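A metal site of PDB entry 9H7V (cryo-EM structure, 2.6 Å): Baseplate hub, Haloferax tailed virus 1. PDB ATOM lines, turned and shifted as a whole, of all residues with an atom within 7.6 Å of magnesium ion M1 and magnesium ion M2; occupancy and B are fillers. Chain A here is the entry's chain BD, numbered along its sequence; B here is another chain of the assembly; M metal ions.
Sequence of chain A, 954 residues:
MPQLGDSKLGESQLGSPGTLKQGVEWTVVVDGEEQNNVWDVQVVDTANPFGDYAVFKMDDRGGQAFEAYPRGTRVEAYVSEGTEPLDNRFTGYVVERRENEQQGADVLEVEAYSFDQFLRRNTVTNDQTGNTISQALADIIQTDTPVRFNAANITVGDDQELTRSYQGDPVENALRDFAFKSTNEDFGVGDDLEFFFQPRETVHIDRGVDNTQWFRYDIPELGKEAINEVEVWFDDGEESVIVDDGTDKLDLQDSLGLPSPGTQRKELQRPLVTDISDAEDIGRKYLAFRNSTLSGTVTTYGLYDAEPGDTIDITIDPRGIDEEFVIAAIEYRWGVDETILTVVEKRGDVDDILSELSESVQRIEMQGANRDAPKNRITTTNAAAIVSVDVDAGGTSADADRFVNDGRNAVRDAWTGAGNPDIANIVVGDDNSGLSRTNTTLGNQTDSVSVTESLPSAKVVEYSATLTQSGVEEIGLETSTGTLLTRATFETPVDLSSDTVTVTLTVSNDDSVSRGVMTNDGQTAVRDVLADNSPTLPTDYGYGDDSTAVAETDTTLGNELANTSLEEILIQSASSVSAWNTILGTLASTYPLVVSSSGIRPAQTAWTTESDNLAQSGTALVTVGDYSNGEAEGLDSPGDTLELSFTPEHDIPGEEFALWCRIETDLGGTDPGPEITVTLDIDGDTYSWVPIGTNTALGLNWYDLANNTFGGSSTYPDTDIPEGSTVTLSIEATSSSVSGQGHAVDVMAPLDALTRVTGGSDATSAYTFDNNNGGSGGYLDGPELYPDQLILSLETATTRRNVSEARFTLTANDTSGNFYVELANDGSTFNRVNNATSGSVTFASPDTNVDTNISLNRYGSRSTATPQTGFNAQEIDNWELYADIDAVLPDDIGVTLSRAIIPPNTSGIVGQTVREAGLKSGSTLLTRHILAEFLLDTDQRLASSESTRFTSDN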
ATOM      1  N   VAL A  44      -5.685   4.033 -28.022  1.00  0.00           N
ATOM      2  CA  VAL A  44      -4.622   4.878 -28.545  1.00  0.00           C
ATOM      3  C   VAL A  44      -4.713   6.255 -27.900  1.00  0.00           C
ATOM      4  O   VAL A  44      -5.765   6.888 -27.910  1.00  0.00           O
ATOM      5  CB  VAL A  44      -4.634   4.940 -30.086  1.00  0.00           C
ATOM      6  CG1 VAL A  44      -3.513   5.822 -30.630  1.00  0.00           C
ATOM      7  CG2 VAL A  44      -4.545   3.556 -30.708  1.00  0.00           C
ATOM      8  N   ASP A  45      -3.575   6.695 -27.341  1.00  0.00           N
ATOM      9  CA  ASP A  45      -3.416   7.988 -26.692  1.00  0.00           C
ATOM     10  C   ASP A  45      -2.267   8.711 -27.373  1.00  0.00           C
ATOM     11  O   ASP A  45      -1.138   8.237 -27.334  1.00  0.00           O
ATOM     12  CB  ASP A  45      -3.174   7.783 -25.187  1.00  0.00           C
ATOM     13  CG  ASP A  45      -3.247   9.039 -24.337  1.00  0.00           C
ATOM     14  OD1 ASP A  45      -3.588  10.113 -24.888  1.00  0.00           O
ATOM     15  OD2 ASP A  45      -2.963   8.940 -23.129  1.00  0.00           O
ATOM     16  N   THR A  46      -2.566   9.862 -28.007  1.00  0.00           N
ATOM     17  CA  THR A  46      -1.636  10.438 -28.975  1.00  0.00           C
ATOM     18  C   THR A  46      -1.704  11.968 -28.993  1.00  0.00           C
ATOM     19  O   THR A  46      -2.788  12.554 -28.876  1.00  0.00           O
ATOM     20  CB  THR A  46      -1.787   9.777 -30.349  1.00  0.00           C
ATOM     21  OG1 THR A  46      -0.857  10.361 -31.268  1.00  0.00           O
ATOM     22  CG2 THR A  46      -3.196   9.856 -30.915  1.00  0.00           C
ATOM     23  N   ALA A  47      -0.523  12.571 -29.196  1.00  0.00           N
ATOM     24  CA  ALA A  47      -0.272  14.012 -29.184  1.00  0.00           C
ATOM     25  C   ALA A  47      -1.093  14.721 -30.263  1.00  0.00           C
ATOM     26  O   ALA A  47      -1.597  14.080 -31.190  1.00  0.00           O
ATOM     27  CB  ALA A  47       1.207  14.268 -29.340  1.00  0.00           C
ATOM     28  N   ASN A  48      -1.139  16.057 -30.158  1.00  0.00           N
ATOM     29  CA  ASN A  48      -2.242  16.895 -30.614  1.00  0.00           C
ATOM     30  C   ASN A  48      -2.636  16.704 -32.085  1.00  0.00           C
ATOM     31  O   ASN A  48      -3.838  16.665 -32.340  1.00  0.00           O
ATOM     32  CB  ASN A  48      -2.070  18.361 -30.198  1.00  0.00           C
ATOM     33  CG  ASN A  48      -2.297  18.559 -28.720  1.00  0.00           C
ATOM     34  OD1 ASN A  48      -3.405  18.348 -28.223  1.00  0.00           O
ATOM     35  ND2 ASN A  48      -1.254  18.954 -28.018  1.00  0.00           N
ATOM     36  N   PRO A  49      -1.716  16.620 -33.080  1.00  0.00           N
ATOM     37  CA  PRO A  49      -2.144  16.445 -34.476  1.00  0.00           C
ATOM     38  C   PRO A  49      -3.045  15.228 -34.722  1.00  0.00           C
ATOM     39  O   PRO A  49      -3.718  15.161 -35.743  1.00  0.00           O
ATOM     40  CB  PRO A  49      -0.825  16.282 -35.243  1.00  0.00           C
ATOM     41  CG  PRO A  49       0.195  16.983 -34.379  1.00  0.00           C
ATOM     42  CD  PRO A  49      -0.255  16.731 -32.957  1.00  0.00           C
ATOM     43  N   PHE A  50      -3.070  14.301 -33.750  1.00  0.00           N
ATOM     44  CA  PHE A  50      -3.652  12.978 -33.941  1.00  0.00           C
ATOM     45  C   PHE A  50      -4.766  12.708 -32.920  1.00  0.00           C
ATOM     46  O   PHE A  50      -4.664  13.105 -31.763  1.00  0.00           O
ATOM     47  CB  PHE A  50      -2.571  11.906 -33.884  1.00  0.00           C
ATOM     48  CG  PHE A  50      -1.519  12.036 -34.961  1.00  0.00           C
ATOM     49  CD1 PHE A  50      -1.750  11.550 -36.238  1.00  0.00           C
ATOM     50  CD2 PHE A  50      -0.312  12.659 -34.693  1.00  0.00           C
ATOM     51  CE1 PHE A  50      -0.792  11.679 -37.222  1.00  0.00           C
ATOM     52  CE2 PHE A  50       0.652  12.788 -35.686  1.00  0.00           C
ATOM     53  CZ  PHE A  50       0.408  12.291 -36.959  1.00  0.00           C
ATOM     54  N   GLY A  51      -5.796  11.991 -33.390  1.00  0.00           N
ATOM     55  CA  GLY A  51      -6.981  11.706 -32.610  1.00  0.00           C
ATOM     56  C   GLY A  51      -6.804  10.484 -31.703  1.00  0.00           C
ATOM     57  O   GLY A  51      -6.374   9.431 -32.164  1.00  0.00           O
ATOM     58  N   ASP A  52      -7.136  10.659 -30.417  1.00  0.00           N
ATOM     59  CA  ASP A  52      -7.199   9.571 -29.457  1.00  0.00           C
ATOM     60  C   ASP A  52      -8.448   8.744 -29.750  1.00  0.00           C
ATOM     61  O   ASP A  52      -9.534   9.299 -29.909  1.00  0.00           O
ATOM     62  CB  ASP A  52      -7.223  10.091 -28.022  1.00  0.00           C
ATOM     63  CG  ASP A  52      -6.042  10.955 -27.617  1.00  0.00           C
ATOM     64  OD1 ASP A  52      -5.247  11.338 -28.506  1.00  0.00           O
ATOM     65  OD2 ASP A  52      -5.918  11.240 -26.416  1.00  0.00           O
ATOM     66  N   TYR A  53      -8.276   7.421 -29.822  1.00  0.00           N
ATOM     67  CA  TYR A  53      -9.385   6.539 -30.147  1.00  0.00           C
ATOM     68  C   TYR A  53      -9.276   5.200 -29.413  1.00  0.00           C
ATOM     69  O   TYR A  53      -8.193   4.815 -28.986  1.00  0.00           O
ATOM     70  CB  TYR A  53      -9.528   6.359 -31.666  1.00  0.00           C
ATOM     71  CG  TYR A  53      -8.497   5.480 -32.343  1.00  0.00           C
ATOM     72  CD1 TYR A  53      -7.241   5.964 -32.673  1.00  0.00           C
ATOM     73  CD2 TYR A  53      -8.794   4.169 -32.681  1.00  0.00           C
ATOM     74  CE1 TYR A  53      -6.302   5.169 -33.308  1.00  0.00           C
ATOM     75  CE2 TYR A  53      -7.866   3.353 -33.312  1.00  0.00           C
ATOM     76  CZ  TYR A  53      -6.611   3.858 -33.631  1.00  0.00           C
ATOM     77  OH  TYR A  53      -5.699   3.072 -34.249  1.00  0.00           O
ATOM     78  N   ARG A  89      -8.390   4.515 -18.232  1.00  0.00           N
ATOM     79  CA  ARG A  89      -7.333   4.807 -19.184  1.00  0.00           C
ATOM     80  C   ARG A  89      -7.856   5.528 -20.426  1.00  0.00           C
ATOM     81  O   ARG A  89      -7.098   6.247 -21.077  1.00  0.00           O
ATOM     82  CB  ARG A  89      -6.526   3.543 -19.530  1.00  0.00           C
ATOM     83  CG  ARG A  89      -5.207   3.805 -20.258  1.00  0.00           C
ATOM     84  CD  ARG A  89      -4.323   4.811 -19.542  1.00  0.00           C
ATOM     85  NE  ARG A  89      -3.168   5.311 -20.288  1.00  0.00           N
ATOM     86  CZ  ARG A  89      -3.189   6.305 -21.171  1.00  0.00           C
ATOM     87  NH1 ARG A  89      -2.065   6.657 -21.773  1.00  0.00           N
ATOM     88  NH2 ARG A  89      -4.312   6.926 -21.473  1.00  0.00           N
ATOM     89  N   SER A 114     -12.293  10.747 -28.536  1.00  0.00           N
ATOM     90  CA  SER A 114     -12.156  11.414 -27.248  1.00  0.00           C
ATOM     91  C   SER A 114     -12.215  12.937 -27.396  1.00  0.00           C
ATOM     92  O   SER A 114     -12.688  13.444 -28.408  1.00  0.00           O
ATOM     93  CB  SER A 114     -10.910  10.943 -26.531  1.00  0.00           C
ATOM     94  OG  SER A 114     -10.949  11.299 -25.154  1.00  0.00           O
ATOM     95  N   PHE A 115     -11.727  13.651 -26.371  1.00  0.00           N
ATOM     96  CA  PHE A 115     -11.983  15.074 -26.152  1.00  0.00           C
ATOM     97  C   PHE A 115     -11.200  15.967 -27.102  1.00  0.00           C
ATOM     98  O   PHE A 115     -11.560  17.135 -27.268  1.00  0.00           O
ATOM     99  CB  PHE A 115     -11.720  15.467 -24.698  1.00  0.00           C
ATOM    100  CG  PHE A 115     -12.530  14.679 -23.696  1.00  0.00           C
ATOM    101  CD1 PHE A 115     -13.880  14.958 -23.508  1.00  0.00           C
ATOM    102  CD2 PHE A 115     -11.945  13.647 -22.975  1.00  0.00           C
ATOM    103  CE1 PHE A 115     -14.624  14.218 -22.596  1.00  0.00           C
ATOM    104  CE2 PHE A 115     -12.698  12.915 -22.070  1.00  0.00           C
ATOM    105  CZ  PHE A 115     -14.034  13.196 -21.883  1.00  0.00           C
ATOM    106  N   ASP A 116     -10.136  15.439 -27.725  1.00  0.00           N
ATOM    107  CA  ASP A 116      -9.294  16.239 -28.602  1.00  0.00           C
ATOM    108  C   ASP A 116     -10.043  16.614 -29.881  1.00  0.00           C
ATOM    109  O   ASP A 116      -9.616  17.505 -30.611  1.00  0.00           O
ATOM    110  CB  ASP A 116      -7.864  15.683 -28.748  1.00  0.00           C
ATOM    111  CG  ASP A 116      -7.705  14.357 -29.469  1.00  0.00           C
ATOM    112  OD1 ASP A 116      -8.721  13.762 -29.881  1.00  0.00           O
ATOM    113  OD2 ASP A 116      -6.536  13.913 -29.614  1.00  0.00           O
ATOM    114  N   GLN A 117     -11.187  15.944 -30.113  1.00  0.00           N
ATOM    115  CA  GLN A 117     -12.072  16.207 -31.240  1.00  0.00           C
ATOM    116  C   GLN A 117     -12.670  17.609 -31.154  1.00  0.00           C
ATOM    117  O   GLN A 117     -12.930  18.216 -32.195  1.00  0.00           O
ATOM    118  CB  GLN A 117     -13.171  15.146 -31.326  1.00  0.00           C
ATOM    119  CG  GLN A 117     -12.690  13.776 -31.778  1.00  0.00           C
ATOM    120  CD  GLN A 117     -12.081  13.742 -33.160  1.00  0.00           C
ATOM    121  OE1 GLN A 117     -12.493  14.447 -34.067  1.00  0.00           O
ATOM    122  NE2 GLN A 117     -11.071  12.893 -33.326  1.00  0.00           N
ATOM    123  N   ARG A 120     -10.412  20.297 -32.367  1.00  0.00           N
ATOM    124  CA  ARG A 120     -10.110  20.010 -33.761  1.00  0.00           C
ATOM    125  C   ARG A 120     -11.250  20.502 -34.661  1.00  0.00           C
ATOM    126  O   ARG A 120     -11.001  21.028 -35.741  1.00  0.00           O
ATOM    127  CB  ARG A 120      -9.950  18.494 -33.887  1.00  0.00           C
ATOM    128  CG  ARG A 120      -9.310  17.997 -35.182  1.00  0.00           C
ATOM    129  CD  ARG A 120      -8.815  16.574 -35.020  1.00  0.00           C
ATOM    130  NE  ARG A 120      -7.697  16.503 -34.085  1.00  0.00           N
ATOM    131  CZ  ARG A 120      -7.566  15.647 -33.073  1.00  0.00           C
ATOM    132  NH1 ARG A 120      -6.497  15.698 -32.304  1.00  0.00           N
ATOM    133  NH2 ARG A 120      -8.491  14.720 -32.843  1.00  0.00           N
ATOM    134  N   GLU A 172      -7.090  23.881 -32.689  1.00  0.00           N
ATOM    135  CA  GLU A 172      -5.887  23.063 -32.560  1.00  0.00           C
ATOM    136  C   GLU A 172      -4.732  23.646 -33.370  1.00  0.00           C
ATOM    137  O   GLU A 172      -3.583  23.613 -32.915  1.00  0.00           O
ATOM    138  CB  GLU A 172      -6.210  21.618 -32.952  1.00  0.00           C
ATOM    139  CG  GLU A 172      -5.082  20.632 -32.700  1.00  0.00           C
ATOM    140  CD  GLU A 172      -5.287  19.320 -33.433  1.00  0.00           C
ATOM    141  OE1 GLU A 172      -6.104  18.503 -32.975  1.00  0.00           O
ATOM    142  OE2 GLU A 172      -4.637  19.134 -34.491  1.00  0.00           O
ATOM    143  N   PHE A 187      -0.191  20.924 -25.063  1.00  0.00           N
ATOM    144  CA  PHE A 187      -1.564  21.310 -24.745  1.00  0.00           C
ATOM    145  C   PHE A 187      -2.491  20.111 -24.911  1.00  0.00           C
ATOM    146  O   PHE A 187      -2.106  19.080 -25.456  1.00  0.00           O
ATOM    147  CB  PHE A 187      -2.002  22.535 -25.561  1.00  0.00           C
ATOM    148  CG  PHE A 187      -2.072  22.330 -27.050  1.00  0.00           C
ATOM    149  CD1 PHE A 187      -3.257  21.917 -27.658  1.00  0.00           C
ATOM    150  CD2 PHE A 187      -0.971  22.568 -27.854  1.00  0.00           C
ATOM    151  CE1 PHE A 187      -3.320  21.740 -29.029  1.00  0.00           C
ATOM    152  CE2 PHE A 187      -1.033  22.382 -29.224  1.00  0.00           C
ATOM    153  CZ  PHE A 187      -2.208  21.972 -29.813  1.00  0.00           C
ATOM    154  N   GLY A 188      -3.722  20.278 -24.416  1.00  0.00           N
ATOM    155  CA  GLY A 188      -4.762  19.276 -24.585  1.00  0.00           C
ATOM    156  C   GLY A 188      -5.830  19.380 -23.502  1.00  0.00           C
ATOM    157  O   GLY A 188      -5.872  20.351 -22.745  1.00  0.00           O
ATOM    158  N   VAL A 189      -6.682  18.356 -23.453  1.00  0.00           N
ATOM    159  CA  VAL A 189      -7.735  18.233 -22.465  1.00  0.00           C
ATOM    160  C   VAL A 189      -7.355  17.076 -21.544  1.00  0.00           C
ATOM    161  O   VAL A 189      -7.152  15.948 -21.999  1.00  0.00           O
ATOM    162  CB  VAL A 189      -9.111  18.008 -23.122  1.00  0.00           C
ATOM    163  CG1 VAL A 189     -10.236  17.981 -22.104  1.00  0.00           C
ATOM    164  CG2 VAL A 189      -9.403  19.034 -24.199  1.00  0.00           C
ATOM    165  N   ASP A 191      -8.013  14.466 -18.096  1.00  0.00           N
ATOM    166  CA  ASP A 191      -9.067  13.539 -17.726  1.00  0.00           C
ATOM    167  C   ASP A 191     -10.200  14.267 -16.997  1.00  0.00           C
ATOM    168  O   ASP A 191     -11.342  13.822 -17.020  1.00  0.00           O
ATOM    169  CB  ASP A 191      -8.519  12.387 -16.879  1.00  0.00           C
ATOM    170  CG  ASP A 191      -7.476  11.520 -17.559  1.00  0.00           C
ATOM    171  OD1 ASP A 191      -7.459  11.475 -18.811  1.00  0.00           O
ATOM    172  OD2 ASP A 191      -6.677  10.888 -16.837  1.00  0.00           O
ATOM    173  N   PHE A 196      -5.139  22.335 -20.617  1.00  0.00           N
ATOM    174  CA  PHE A 196      -3.814  22.680 -20.139  1.00  0.00           C
ATOM    175  C   PHE A 196      -2.953  23.187 -21.295  1.00  0.00           C
ATOM    176  O   PHE A 196      -3.171  22.805 -22.440  1.00  0.00           O
ATOM    177  CB  PHE A 196      -3.156  21.508 -19.396  1.00  0.00           C
ATOM    178  CG  PHE A 196      -2.838  20.300 -20.251  1.00  0.00           C
ATOM    179  CD1 PHE A 196      -1.626  20.197 -20.912  1.00  0.00           C
ATOM    180  CD2 PHE A 196      -3.741  19.255 -20.366  1.00  0.00           C
ATOM    181  CE1 PHE A 196      -1.333  19.086 -21.700  1.00  0.00           C
ATOM    182  CE2 PHE A 196      -3.453  18.144 -21.145  1.00  0.00           C
ATOM    183  CZ  PHE A 196      -2.245  18.061 -21.810  1.00  0.00           C
ATOM    184  N   GLU A 307       1.736   8.616 -20.410  1.00  0.00           N
ATOM    185  CA  GLU A 307       0.993   9.474 -21.321  1.00  0.00           C
ATOM    186  C   GLU A 307       1.943   9.996 -22.398  1.00  0.00           C
ATOM    187  O   GLU A 307       3.152   9.977 -22.198  1.00  0.00           O
ATOM    188  CB  GLU A 307       0.372  10.633 -20.556  1.00  0.00           C
ATOM    189  CG  GLU A 307      -0.870  10.260 -19.754  1.00  0.00           C
ATOM    190  CD  GLU A 307      -1.535  11.399 -19.009  1.00  0.00           C
ATOM    191  OE1 GLU A 307      -1.565  12.523 -19.551  1.00  0.00           O
ATOM    192  OE2 GLU A 307      -2.018  11.160 -17.888  1.00  0.00           O
ATOM    193  N   PRO A 308       1.441  10.476 -23.567  1.00  0.00           N
ATOM    194  CA  PRO A 308       2.264  11.268 -24.484  1.00  0.00           C
ATOM    195  C   PRO A 308       2.686  12.564 -23.813  1.00  0.00           C
ATOM    196  O   PRO A 308       1.905  13.192 -23.091  1.00  0.00           O
ATOM    197  CB  PRO A 308       1.367  11.515 -25.708  1.00  0.00           C
ATOM    198  CG  PRO A 308      -0.039  11.280 -25.196  1.00  0.00           C
ATOM    199  CD  PRO A 308       0.092  10.242 -24.104  1.00  0.00           C
ATOM    200  N   ALA A 328       5.501  10.197 -27.939  1.00  0.00           N
ATOM    201  CA  ALA A 328       4.618  10.910 -28.851  1.00  0.00           C
ATOM    202  C   ALA A 328       3.230  10.276 -28.854  1.00  0.00           C
ATOM    203  O   ALA A 328       2.231  10.976 -29.027  1.00  0.00           O
ATOM    204  CB  ALA A 328       5.222  10.928 -30.226  1.00  0.00           C
ATOM    205  N   ARG B 338     -10.266  10.710 -37.986  1.00  0.00           N
ATOM    206  CA  ARG B 338      -9.769  11.038 -36.667  1.00  0.00           C
ATOM    207  C   ARG B 338      -9.237  12.466 -36.617  1.00  0.00           C
ATOM    208  O   ARG B 338      -9.221  13.081 -35.557  1.00  0.00           O
ATOM    209  CB  ARG B 338      -8.667  10.051 -36.258  1.00  0.00           C
ATOM    210  CG  ARG B 338      -9.143   8.935 -35.333  1.00  0.00           C
ATOM    211  CD  ARG B 338      -8.617   7.560 -35.725  1.00  0.00           C
ATOM    212  NE  ARG B 338      -7.162   7.475 -35.815  1.00  0.00           N
ATOM    213  CZ  ARG B 338      -6.488   6.460 -36.343  1.00  0.00           C
ATOM    214  NH1 ARG B 338      -5.167   6.488 -36.361  1.00  0.00           N
ATOM    215  NH2 ARG B 338      -7.126   5.411 -36.846  1.00  0.00           N
HETATM  216 MG    MG M   1      -4.728  13.021 -29.653  1.00  0.00          MG
HETATM  217 MG    MG M   2      -4.093  12.289 -25.129  1.00  0.00          MG
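Of the 26 residues printed, 3 come within 4 Å of magnesium ion M2.
Merely in contact with magnesium ion M1: Ala 47 (3.6 Å) and Gly 51 (3.9 Å).
The nearest printed residue that does not touch magnesium ion M1 is Arg 120 (4.2 Å).
The side-chain carboxylate (OD1) of Asp 45 binds magnesium ion M2.
OD2 of Asp 52 binds magnesium ion M2 (2.5 Å).
OD2 of Asp 116 binds magnesium ion M1 (2.0 Å).
The side-chain carboxylate (OD1) of Asp 52 binds magnesium ion M1 (2.1 Å).
O of Phe 50 is bound to magnesium ion M1 (2.1 Å).
The backbone carbonyl oxygen (O) of Thr 46 binds magnesium ion M1 (2.1 Å).
The guanidinium group (NH2) of Arg 120 lies within salt-bridge range of the side-chain carboxylate (OD1) of Asp 116 (3.1 Å).
The backbone carbonyl oxygen of Asp 52 sits at hydrogen-bond distance from the backbone NH of Ser 114, at 3.4 Å.
O of Phe 50 lies close to NH1 of Arg 120 (3.2 Å).
The guanidinium group (NH1) of Arg 89 lies within salt-bridge range of the side-chain carboxylate (OD2) of Asp 45 (2.8 Å).
O of Ala 328 lies within hydrogen-bond range of N of Ala 47 (3.2 Å).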
